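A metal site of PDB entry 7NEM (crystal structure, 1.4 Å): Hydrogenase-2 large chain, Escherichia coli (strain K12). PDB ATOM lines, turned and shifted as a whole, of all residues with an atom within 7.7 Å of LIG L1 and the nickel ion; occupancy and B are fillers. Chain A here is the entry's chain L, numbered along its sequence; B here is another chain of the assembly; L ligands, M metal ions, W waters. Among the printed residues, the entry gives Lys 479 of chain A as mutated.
SG of Cys 546 sits close to OE1 of Glu 14 (3.5 Å). The backbone NH (N) of Cys 546 sits at hydrogen-bond distance from the side-chain hydroxyl (OG) of Ser 502, 3.2 Å away. O of Cys 64 sits at hydrogen-bond distance from OG1 of Thr 67 (2.8 Å). NE2 of His 68 sits close to SG of Cys 549. The side-chain sulfur of Cys 61 lies close to the backbone NH of Val 63, at 3.4 Å. NZ of Lys 479 lies within salt-bridge range of OD1 of Asp 103, 2.7 Å away. NZ of Lys 479 lies within salt-bridge range of OD2 of Asp 544. The backbone carbonyl oxygen of Val 63 sits close to a ring nitrogen (NE2) of His 99, at 3.3 Å.
Residues that only touch LIG L1: Val 63 (3.2 Å). Hydrophobic or aromatic side chains that line LIG L1: Val 63.
The nickel ion is bound by O2 of LIG L1 (1.8 Å), SG of Cys 546 (2.2 Å), SG of Cys 64 (2.3 Å), SG of Cys 549 (2.3 Å) and SG of Cys 61 (2.3 Å).
O2 of LIG L1 sits close to N of Cys 64, at 3.5 Å. The side-chain amino group (NZ) of Lys 479 lies within hydrogen-bond range of an oxygen (O1) of LIG L1, 2.7 Å away. FE1 of LG2 L2 is bound by SG of Cys 64, 2.2 Å away. SG of Cys 549 is bound to FE1 of LG2 L2, 2.3 Å away. The backbone NH of Lys 479 lies within hydrogen-bond range of a nitrogen (N2) of LG2 L2 (2.9 Å). A ring nitrogen (NE2) of His 68 lies close to an oxygen (O1) of LG2 L2 (3.5 Å). N of Ser 502 is in hydrogen-bond range of N1 of LG2 L2, at 3.1 Å. The side-chain hydroxyl (OG) of Ser 502 is in hydrogen-bond range of a nitrogen (N1) of LG2 L2 (2.8 Å).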
ATOM      1  N   ILE A  13      15.268  -7.926   0.576  1.00  0.00           N
ATOM      2  CA  ILE A  13      15.358  -7.002   1.701  1.00  0.00           C
ATOM      3  C   ILE A  13      16.836  -6.852   2.051  1.00  0.00           C
ATOM      4  O   ILE A  13      17.686  -7.564   1.482  1.00  0.00           O
ATOM      5  CB  ILE A  13      14.587  -7.540   2.915  1.00  0.00           C
ATOM      6  CG1 ILE A  13      15.170  -8.849   3.431  1.00  0.00           C
ATOM      7  CG2 ILE A  13      13.093  -7.695   2.619  1.00  0.00           C
ATOM      8  CD1 ILE A  13      14.697  -9.198   4.822  1.00  0.00           C
ATOM      9  N   GLU A  14      17.140  -6.023   3.032  1.00  0.00           N
ATOM     10  CA  GLU A  14      18.440  -6.120   3.708  1.00  0.00           C
ATOM     11  C   GLU A  14      18.338  -7.122   4.875  1.00  0.00           C
ATOM     12  O   GLU A  14      17.441  -6.949   5.759  1.00  0.00           O
ATOM     13  CB  GLU A  14      18.889  -4.753   4.179  1.00  0.00           C
ATOM     14  CG  GLU A  14      20.309  -4.780   4.694  1.00  0.00           C
ATOM     15  CD  GLU A  14      20.619  -5.638   5.909  1.00  0.00           C
ATOM     16  OE1 GLU A  14      19.774  -5.726   6.787  1.00  0.00           O
ATOM     17  OE2 GLU A  14      21.765  -6.237   5.986  1.00  0.00           O
ATOM     18  N   ILE A  60      26.369  -0.735  11.242  1.00  0.00           N
ATOM     19  CA  ILE A  60      25.061  -1.358  11.482  1.00  0.00           C
ATOM     20  C   ILE A  60      24.457  -1.723  10.132  1.00  0.00           C
ATOM     21  O   ILE A  60      23.833  -2.810  10.025  1.00  0.00           O
ATOM     22  CB  ILE A  60      24.121  -0.439  12.274  1.00  0.00           C
ATOM     23  CG1 ILE A  60      24.563  -0.442  13.755  1.00  0.00           C
ATOM     24  CG2 ILE A  60      22.691  -0.879  12.122  1.00  0.00           C
ATOM     25  CD1 ILE A  60      23.919   0.609  14.615  1.00  0.00           C
ATOM     26  N   CYS A  61      24.635  -0.898   9.103  1.00  0.00           N
ATOM     27  CA  CYS A  61      23.966  -1.198   7.818  1.00  0.00           C
ATOM     28  C   CYS A  61      24.711  -0.535   6.666  1.00  0.00           C
ATOM     29  O   CYS A  61      25.034   0.662   6.749  1.00  0.00           O
ATOM     30  CB  CYS A  61      22.520  -0.761   7.862  1.00  0.00           C
ATOM     31  SG  CYS A  61      21.581  -1.250   6.394  1.00  0.00           S
ATOM     32  N   GLY A  62      24.888  -1.329   5.614  1.00  0.00           N
ATOM     33  CA  GLY A  62      25.493  -0.838   4.373  1.00  0.00           C
ATOM     34  C   GLY A  62      24.495  -0.519   3.293  1.00  0.00           C
ATOM     35  O   GLY A  62      24.968   0.004   2.255  1.00  0.00           O
ATOM     36  N   VAL A  63      23.210  -0.832   3.456  1.00  0.00           N
ATOM     37  CA  VAL A  63      22.177  -0.349   2.528  1.00  0.00           C
ATOM     38  C   VAL A  63      21.904   1.091   2.934  1.00  0.00           C
ATOM     39  O   VAL A  63      22.152   1.999   2.124  1.00  0.00           O
ATOM     40  CB  VAL A  63      20.926  -1.212   2.540  1.00  0.00           C
ATOM     41  CG1 VAL A  63      19.845  -0.592   1.652  1.00  0.00           C
ATOM     42  CG2 VAL A  63      21.278  -2.596   2.061  1.00  0.00           C
ATOM     43  N   CYS A  64      21.480   1.330   4.170  1.00  0.00           N
ATOM     44  CA  CYS A  64      21.289   2.697   4.687  1.00  0.00           C
ATOM     45  C   CYS A  64      22.619   3.146   5.265  1.00  0.00           C
ATOM     46  O   CYS A  64      22.695   3.658   6.361  1.00  0.00           O
ATOM     47  CB  CYS A  64      20.105   2.802   5.637  1.00  0.00           C
ATOM     48  SG  CYS A  64      20.252   1.813   7.152  1.00  0.00           S
ATOM     49  N   THR A  65      23.658   3.031   4.440  1.00  0.00           N
ATOM     50  CA  THR A  65      24.947   3.658   4.767  1.00  0.00           C
ATOM     51  C   THR A  65      24.684   5.161   4.911  1.00  0.00           C
ATOM     52  O   THR A  65      23.653   5.658   4.458  1.00  0.00           O
ATOM     53  CB  THR A  65      26.007   3.226   3.763  1.00  0.00           C
ATOM     54  OG1 THR A  65      27.274   3.687   4.259  1.00  0.00           O
ATOM     55  CG2 THR A  65      25.763   3.796   2.393  1.00  0.00           C
ATOM     56  N   THR A  67      23.525   6.775   7.307  1.00  0.00           N
ATOM     57  CA  THR A  67      22.494   7.185   8.275  1.00  0.00           C
ATOM     58  C   THR A  67      22.979   7.018   9.722  1.00  0.00           C
ATOM     59  O   THR A  67      22.746   7.940  10.578  1.00  0.00           O
ATOM     60  CB  THR A  67      21.166   6.440   8.068  1.00  0.00           C
ATOM     61  OG1 THR A  67      21.300   5.049   8.352  1.00  0.00           O
ATOM     62  CG2 THR A  67      20.653   6.692   6.670  1.00  0.00           C
ATOM     63  N   HIS A  68      23.529   5.874  10.027  1.00  0.00           N
ATOM     64  CA  HIS A  68      23.968   5.615  11.408  1.00  0.00           C
ATOM     65  C   HIS A  68      25.211   6.451  11.738  1.00  0.00           C
ATOM     66  O   HIS A  68      25.386   6.837  12.924  1.00  0.00           O
ATOM     67  CB  HIS A  68      24.273   4.131  11.588  1.00  0.00           C
ATOM     68  CG  HIS A  68      23.054   3.305  11.506  1.00  0.00           C
ATOM     69  ND1 HIS A  68      22.103   3.289  12.536  1.00  0.00           N
ATOM     70  CD2 HIS A  68      22.553   2.532  10.500  1.00  0.00           C
ATOM     71  CE1 HIS A  68      21.108   2.511  12.160  1.00  0.00           C
ATOM     72  NE2 HIS A  68      21.332   2.059  10.916  1.00  0.00           N
ATOM     73  N   HIS A  99      22.135   9.975  -0.900  1.00  0.00           N
ATOM     74  CA  HIS A  99      22.089   8.568  -0.479  1.00  0.00           C
ATOM     75  C   HIS A  99      20.647   8.065  -0.514  1.00  0.00           C
ATOM     76  O   HIS A  99      20.360   6.981  -1.045  1.00  0.00           O
ATOM     77  CB  HIS A  99      22.634   8.381   0.957  1.00  0.00           C
ATOM     78  CG  HIS A  99      22.274   6.998   1.359  1.00  0.00           C
ATOM     79  ND1 HIS A  99      23.005   5.928   0.930  1.00  0.00           N
ATOM     80  CD2 HIS A  99      21.147   6.533   1.948  1.00  0.00           C
ATOM     81  CE1 HIS A  99      22.371   4.854   1.346  1.00  0.00           C
ATOM     82  NE2 HIS A  99      21.209   5.166   1.913  1.00  0.00           N
ATOM     83  N   ASP A 103      18.770   4.980  -2.399  1.00  0.00           N
ATOM     84  CA  ASP A 103      18.129   3.972  -1.565  1.00  0.00           C
ATOM     85  C   ASP A 103      16.714   3.721  -2.090  1.00  0.00           C
ATOM     86  O   ASP A 103      16.310   2.570  -2.301  1.00  0.00           O
ATOM     87  CB  ASP A 103      18.245   4.526  -0.144  1.00  0.00           C
ATOM     88  CG  ASP A 103      18.046   3.507   0.953  1.00  0.00           C
ATOM     89  OD1 ASP A 103      17.051   2.764   0.854  1.00  0.00           O
ATOM     90  OD2 ASP A 103      18.800   3.533   1.925  1.00  0.00           O
ATOM     91  N   HIS A 107      15.115   0.377  -3.882  1.00  0.00           N
ATOM     92  CA  HIS A 107      14.020  -0.338  -3.208  1.00  0.00           C
ATOM     93  C   HIS A 107      12.860  -0.557  -4.185  1.00  0.00           C
ATOM     94  O   HIS A 107      12.288  -1.674  -4.258  1.00  0.00           O
ATOM     95  CB  HIS A 107      13.500   0.395  -1.986  1.00  0.00           C
ATOM     96  CG  HIS A 107      12.438  -0.431  -1.317  1.00  0.00           C
ATOM     97  ND1 HIS A 107      11.103  -0.080  -1.415  1.00  0.00           N
ATOM     98  CD2 HIS A 107      12.524  -1.645  -0.699  1.00  0.00           C
ATOM     99  CE1 HIS A 107      10.402  -1.031  -0.801  1.00  0.00           C
ATOM    100  NE2 HIS A 107      11.233  -2.027  -0.345  1.00  0.00           N
ATOM    101  N   LEU A 111      14.495  -4.195  -5.416  1.00  0.00           N
ATOM    102  CA  LEU A 111      13.946  -4.999  -4.282  1.00  0.00           C
ATOM    103  C   LEU A 111      12.450  -5.288  -4.471  1.00  0.00           C
ATOM    104  O   LEU A 111      12.046  -6.435  -4.186  1.00  0.00           O
ATOM    105  CB  LEU A 111      14.256  -4.313  -2.940  1.00  0.00           C
ATOM    106  CG  LEU A 111      15.737  -4.010  -2.684  1.00  0.00           C
ATOM    107  CD1 LEU A 111      15.947  -3.399  -1.324  1.00  0.00           C
ATOM    108  CD2 LEU A 111      16.582  -5.264  -2.810  1.00  0.00           C
ATOM    109  N   ALA A 477      15.672   8.864   8.357  1.00  0.00           N
ATOM    110  CA  ALA A 477      16.382   7.937   7.471  1.00  0.00           C
ATOM    111  C   ALA A 477      15.448   7.488   6.357  1.00  0.00           C
ATOM    112  O   ALA A 477      14.230   7.660   6.411  1.00  0.00           O
ATOM    113  CB  ALA A 477      16.916   6.791   8.242  1.00  0.00           C
ATOM    114  N   PRO A 478      15.983   6.796   5.328  1.00  0.00           N
ATOM    115  CA  PRO A 478      15.114   6.328   4.263  1.00  0.00           C
ATOM    116  C   PRO A 478      13.969   5.414   4.714  1.00  0.00           C
ATOM    117  O   PRO A 478      12.896   5.404   4.108  1.00  0.00           O
ATOM    118  CB  PRO A 478      16.101   5.580   3.336  1.00  0.00           C
ATOM    119  CG  PRO A 478      17.397   6.306   3.535  1.00  0.00           C
ATOM    120  CD  PRO A 478      17.419   6.596   5.024  1.00  0.00           C
ATOM    121  N   LYS A 479      14.199   4.657   5.781  1.00  0.00           N
ATOM    122  CA  LYS A 479      13.178   3.765   6.367  1.00  0.00           C
ATOM    123  C   LYS A 479      12.402   4.435   7.498  1.00  0.00           C
ATOM    124  O   LYS A 479      11.476   3.821   8.012  1.00  0.00           O
ATOM    125  CB  LYS A 479      13.773   2.435   6.835  1.00  0.00           C
ATOM    126  CG  LYS A 479      13.750   1.311   5.813  1.00  0.00           C
ATOM    127  CD  LYS A 479      15.056   0.978   5.141  1.00  0.00           C
ATOM    128  CE  LYS A 479      15.556   1.958   4.114  1.00  0.00           C
ATOM    129  NZ  LYS A 479      16.263   1.254   3.008  1.00  0.00           N
ATOM    130  N   VAL A 500      16.036   1.985  15.752  1.00  0.00           N
ATOM    131  CA  VAL A 500      16.203   2.149  14.307  1.00  0.00           C
ATOM    132  C   VAL A 500      14.832   2.034  13.651  1.00  0.00           C
ATOM    133  O   VAL A 500      13.959   1.367  14.198  1.00  0.00           O
ATOM    134  CB  VAL A 500      17.235   1.112  13.829  1.00  0.00           C
ATOM    135  CG1 VAL A 500      17.635   1.279  12.377  1.00  0.00           C
ATOM    136  CG2 VAL A 500      18.475   1.213  14.689  1.00  0.00           C
ATOM    137  N   PRO A 501      14.583   2.684  12.499  1.00  0.00           N
ATOM    138  CA  PRO A 501      13.226   2.658  11.968  1.00  0.00           C
ATOM    139  C   PRO A 501      12.658   1.256  11.738  1.00  0.00           C
ATOM    140  O   PRO A 501      11.515   0.991  12.124  1.00  0.00           O
ATOM    141  CB  PRO A 501      13.280   3.480  10.675  1.00  0.00           C
ATOM    142  CG  PRO A 501      14.739   3.688  10.389  1.00  0.00           C
ATOM    143  CD  PRO A 501      15.409   3.639  11.755  1.00  0.00           C
ATOM    144  N   SER A 502      13.439   0.313  11.205  1.00  0.00           N
ATOM    145  CA  SER A 502      12.925  -1.066  11.017  1.00  0.00           C
ATOM    146  C   SER A 502      12.705  -1.732  12.372  1.00  0.00           C
ATOM    147  O   SER A 502      11.914  -2.678  12.445  1.00  0.00           O
ATOM    148  CB  SER A 502      13.771  -1.917  10.114  1.00  0.00           C
ATOM    149  OG  SER A 502      13.728  -1.434   8.766  1.00  0.00           O
ATOM    150  N   ASP A 544      10.074  -1.748   3.314  1.00  0.00           N
ATOM    151  CA  ASP A 544      11.533  -1.696   3.051  1.00  0.00           C
ATOM    152  C   ASP A 544      12.295  -2.247   4.254  1.00  0.00           C
ATOM    153  O   ASP A 544      13.149  -1.573   4.852  1.00  0.00           O
ATOM    154  CB  ASP A 544      11.876  -0.265   2.654  1.00  0.00           C
ATOM    155  CG  ASP A 544      13.259   0.021   2.166  1.00  0.00           C
ATOM    156  OD1 ASP A 544      14.055  -0.908   1.892  1.00  0.00           O
ATOM    157  OD2 ASP A 544      13.503   1.216   1.991  1.00  0.00           O
ATOM    158  N   PRO A 545      12.115  -3.538   4.582  1.00  0.00           N
ATOM    159  CA  PRO A 545      12.800  -4.096   5.737  1.00  0.00           C
ATOM    160  C   PRO A 545      14.315  -4.025   5.613  1.00  0.00           C
ATOM    161  O   PRO A 545      14.928  -4.374   4.614  1.00  0.00           O
ATOM    162  CB  PRO A 545      12.312  -5.546   5.831  1.00  0.00           C
ATOM    163  CG  PRO A 545      11.021  -5.537   5.048  1.00  0.00           C
ATOM    164  CD  PRO A 545      11.240  -4.531   3.943  1.00  0.00           C
ATOM    165  N   CYS A 546      14.893  -3.674   6.751  1.00  0.00           N
ATOM    166  CA  CYS A 546      16.355  -3.699   6.933  1.00  0.00           C
ATOM    167  C   CYS A 546      16.629  -4.352   8.284  1.00  0.00           C
ATOM    168  O   CYS A 546      16.404  -3.716   9.323  1.00  0.00           O
ATOM    169  CB  CYS A 546      16.924  -2.300   6.866  1.00  0.00           C
ATOM    170  SG  CYS A 546      18.732  -2.398   6.961  1.00  0.00           S
ATOM    171  N   MET A 547      17.061  -5.608   8.287  1.00  0.00           N
ATOM    172  CA  MET A 547      17.152  -6.353   9.568  1.00  0.00           C
ATOM    173  C   MET A 547      18.503  -6.162  10.246  1.00  0.00           C
ATOM    174  O   MET A 547      18.566  -6.313  11.488  1.00  0.00           O
ATOM    175  CB  MET A 547      16.854  -7.849   9.350  1.00  0.00           C
ATOM    176  CG  MET A 547      15.479  -8.067   8.721  1.00  0.00           C
ATOM    177  SD  MET A 547      14.102  -7.096   9.407  1.00  0.00           S
ATOM    178  CE  MET A 547      14.014  -7.820  11.020  1.00  0.00           C
ATOM    179  N   ALA A 548      19.532  -5.808   9.510  1.00  0.00           N
ATOM    180  CA  ALA A 548      20.815  -5.387  10.119  1.00  0.00           C
ATOM    181  C   ALA A 548      20.499  -4.132  10.920  1.00  0.00           C
ATOM    182  O   ALA A 548      20.899  -3.971  12.069  1.00  0.00           O
ATOM    183  CB  ALA A 548      21.866  -5.157   9.065  1.00  0.00           C
ATOM    184  N   CYS A 549      19.728  -3.228  10.322  1.00  0.00           N
ATOM    185  CA  CYS A 549      19.218  -2.039  11.035  1.00  0.00           C
ATOM    186  C   CYS A 549      18.313  -2.434  12.202  1.00  0.00           C
ATOM    187  O   CYS A 549      18.487  -1.896  13.317  1.00  0.00           O
ATOM    188  CB  CYS A 549      18.426  -1.175  10.071  1.00  0.00           C
ATOM    189  SG  CYS A 549      19.473  -0.006   9.209  1.00  0.00           S
ATOM    190  N   ALA A 550      17.333  -3.301  11.975  1.00  0.00           N
ATOM    191  CA  ALA A 550      16.307  -3.539  13.014  1.00  0.00           C
ATOM    192  C   ALA A 550      16.990  -4.070  14.270  1.00  0.00           C
ATOM    193  O   ALA A 550      16.558  -3.737  15.379  1.00  0.00           O
ATOM    194  CB  ALA A 550      15.261  -4.506  12.532  1.00  0.00           C
ATOM    195  N   CYS B  21      26.414  -6.548   6.838  1.00  0.00           N
ATOM    196  CA  CYS B  21      25.624  -5.309   6.826  1.00  0.00           C
ATOM    197  C   CYS B  21      25.063  -5.006   5.455  1.00  0.00           C
ATOM    198  O   CYS B  21      24.327  -4.034   5.336  1.00  0.00           O
ATOM    199  CB  CYS B  21      26.478  -4.147   7.336  1.00  0.00           C
ATOM    200  SG  CYS B  21      27.575  -3.437   6.083  1.00  0.00           S
ATOM    201  N   GLU B  26      26.332  -4.084  -1.713  1.00  0.00           N
ATOM    202  CA  GLU B  26      26.042  -2.729  -2.235  1.00  0.00           C
ATOM    203  C   GLU B  26      27.240  -2.167  -3.004  1.00  0.00           C
ATOM    204  O   GLU B  26      27.049  -1.364  -3.927  1.00  0.00           O
ATOM    205  CB  GLU B  26      25.671  -1.781  -1.085  1.00  0.00           C
ATOM    206  CG  GLU B  26      24.255  -1.992  -0.641  1.00  0.00           C
ATOM    207  CD  GLU B  26      23.208  -1.290  -1.478  1.00  0.00           C
ATOM    208  OE1 GLU B  26      23.551  -0.651  -2.465  1.00  0.00           O
ATOM    209  OE2 GLU B  26      21.988  -1.463  -1.159  1.00  0.00           O
HETATM  210  O1  LIG L   1      18.116  -0.176   4.289  1.00  0.00           O
HETATM  211  O2  LIG L   1      18.552  -0.036   5.408  1.00  0.00           O
HETATM  212 FE1  LG2 L   2      18.290   1.649   8.193  1.00  0.00          FE
HETATM  213  C1  LG2 L   2      16.688   0.993   8.769  1.00  0.00           C
HETATM  214  N1  LG2 L   2      15.677   0.491   9.126  1.00  0.00           N
HETATM  215  C2  LG2 L   2      17.414   2.899   7.125  1.00  0.00           C
HETATM  216  N2  LG2 L   2      16.897   3.753   6.528  1.00  0.00           N
HETATM  217  C3  LG2 L   2      18.401   2.941   9.406  1.00  0.00           C
HETATM  218  O1  LG2 L   2      18.407   3.778  10.199  1.00  0.00           O
HETATM  219 NI    NI M   1      19.514  -0.307   6.929  1.00  0.00          NI
HETATM  220  O   HOH W   1      17.066  -2.432   2.817  1.00  0.00           O
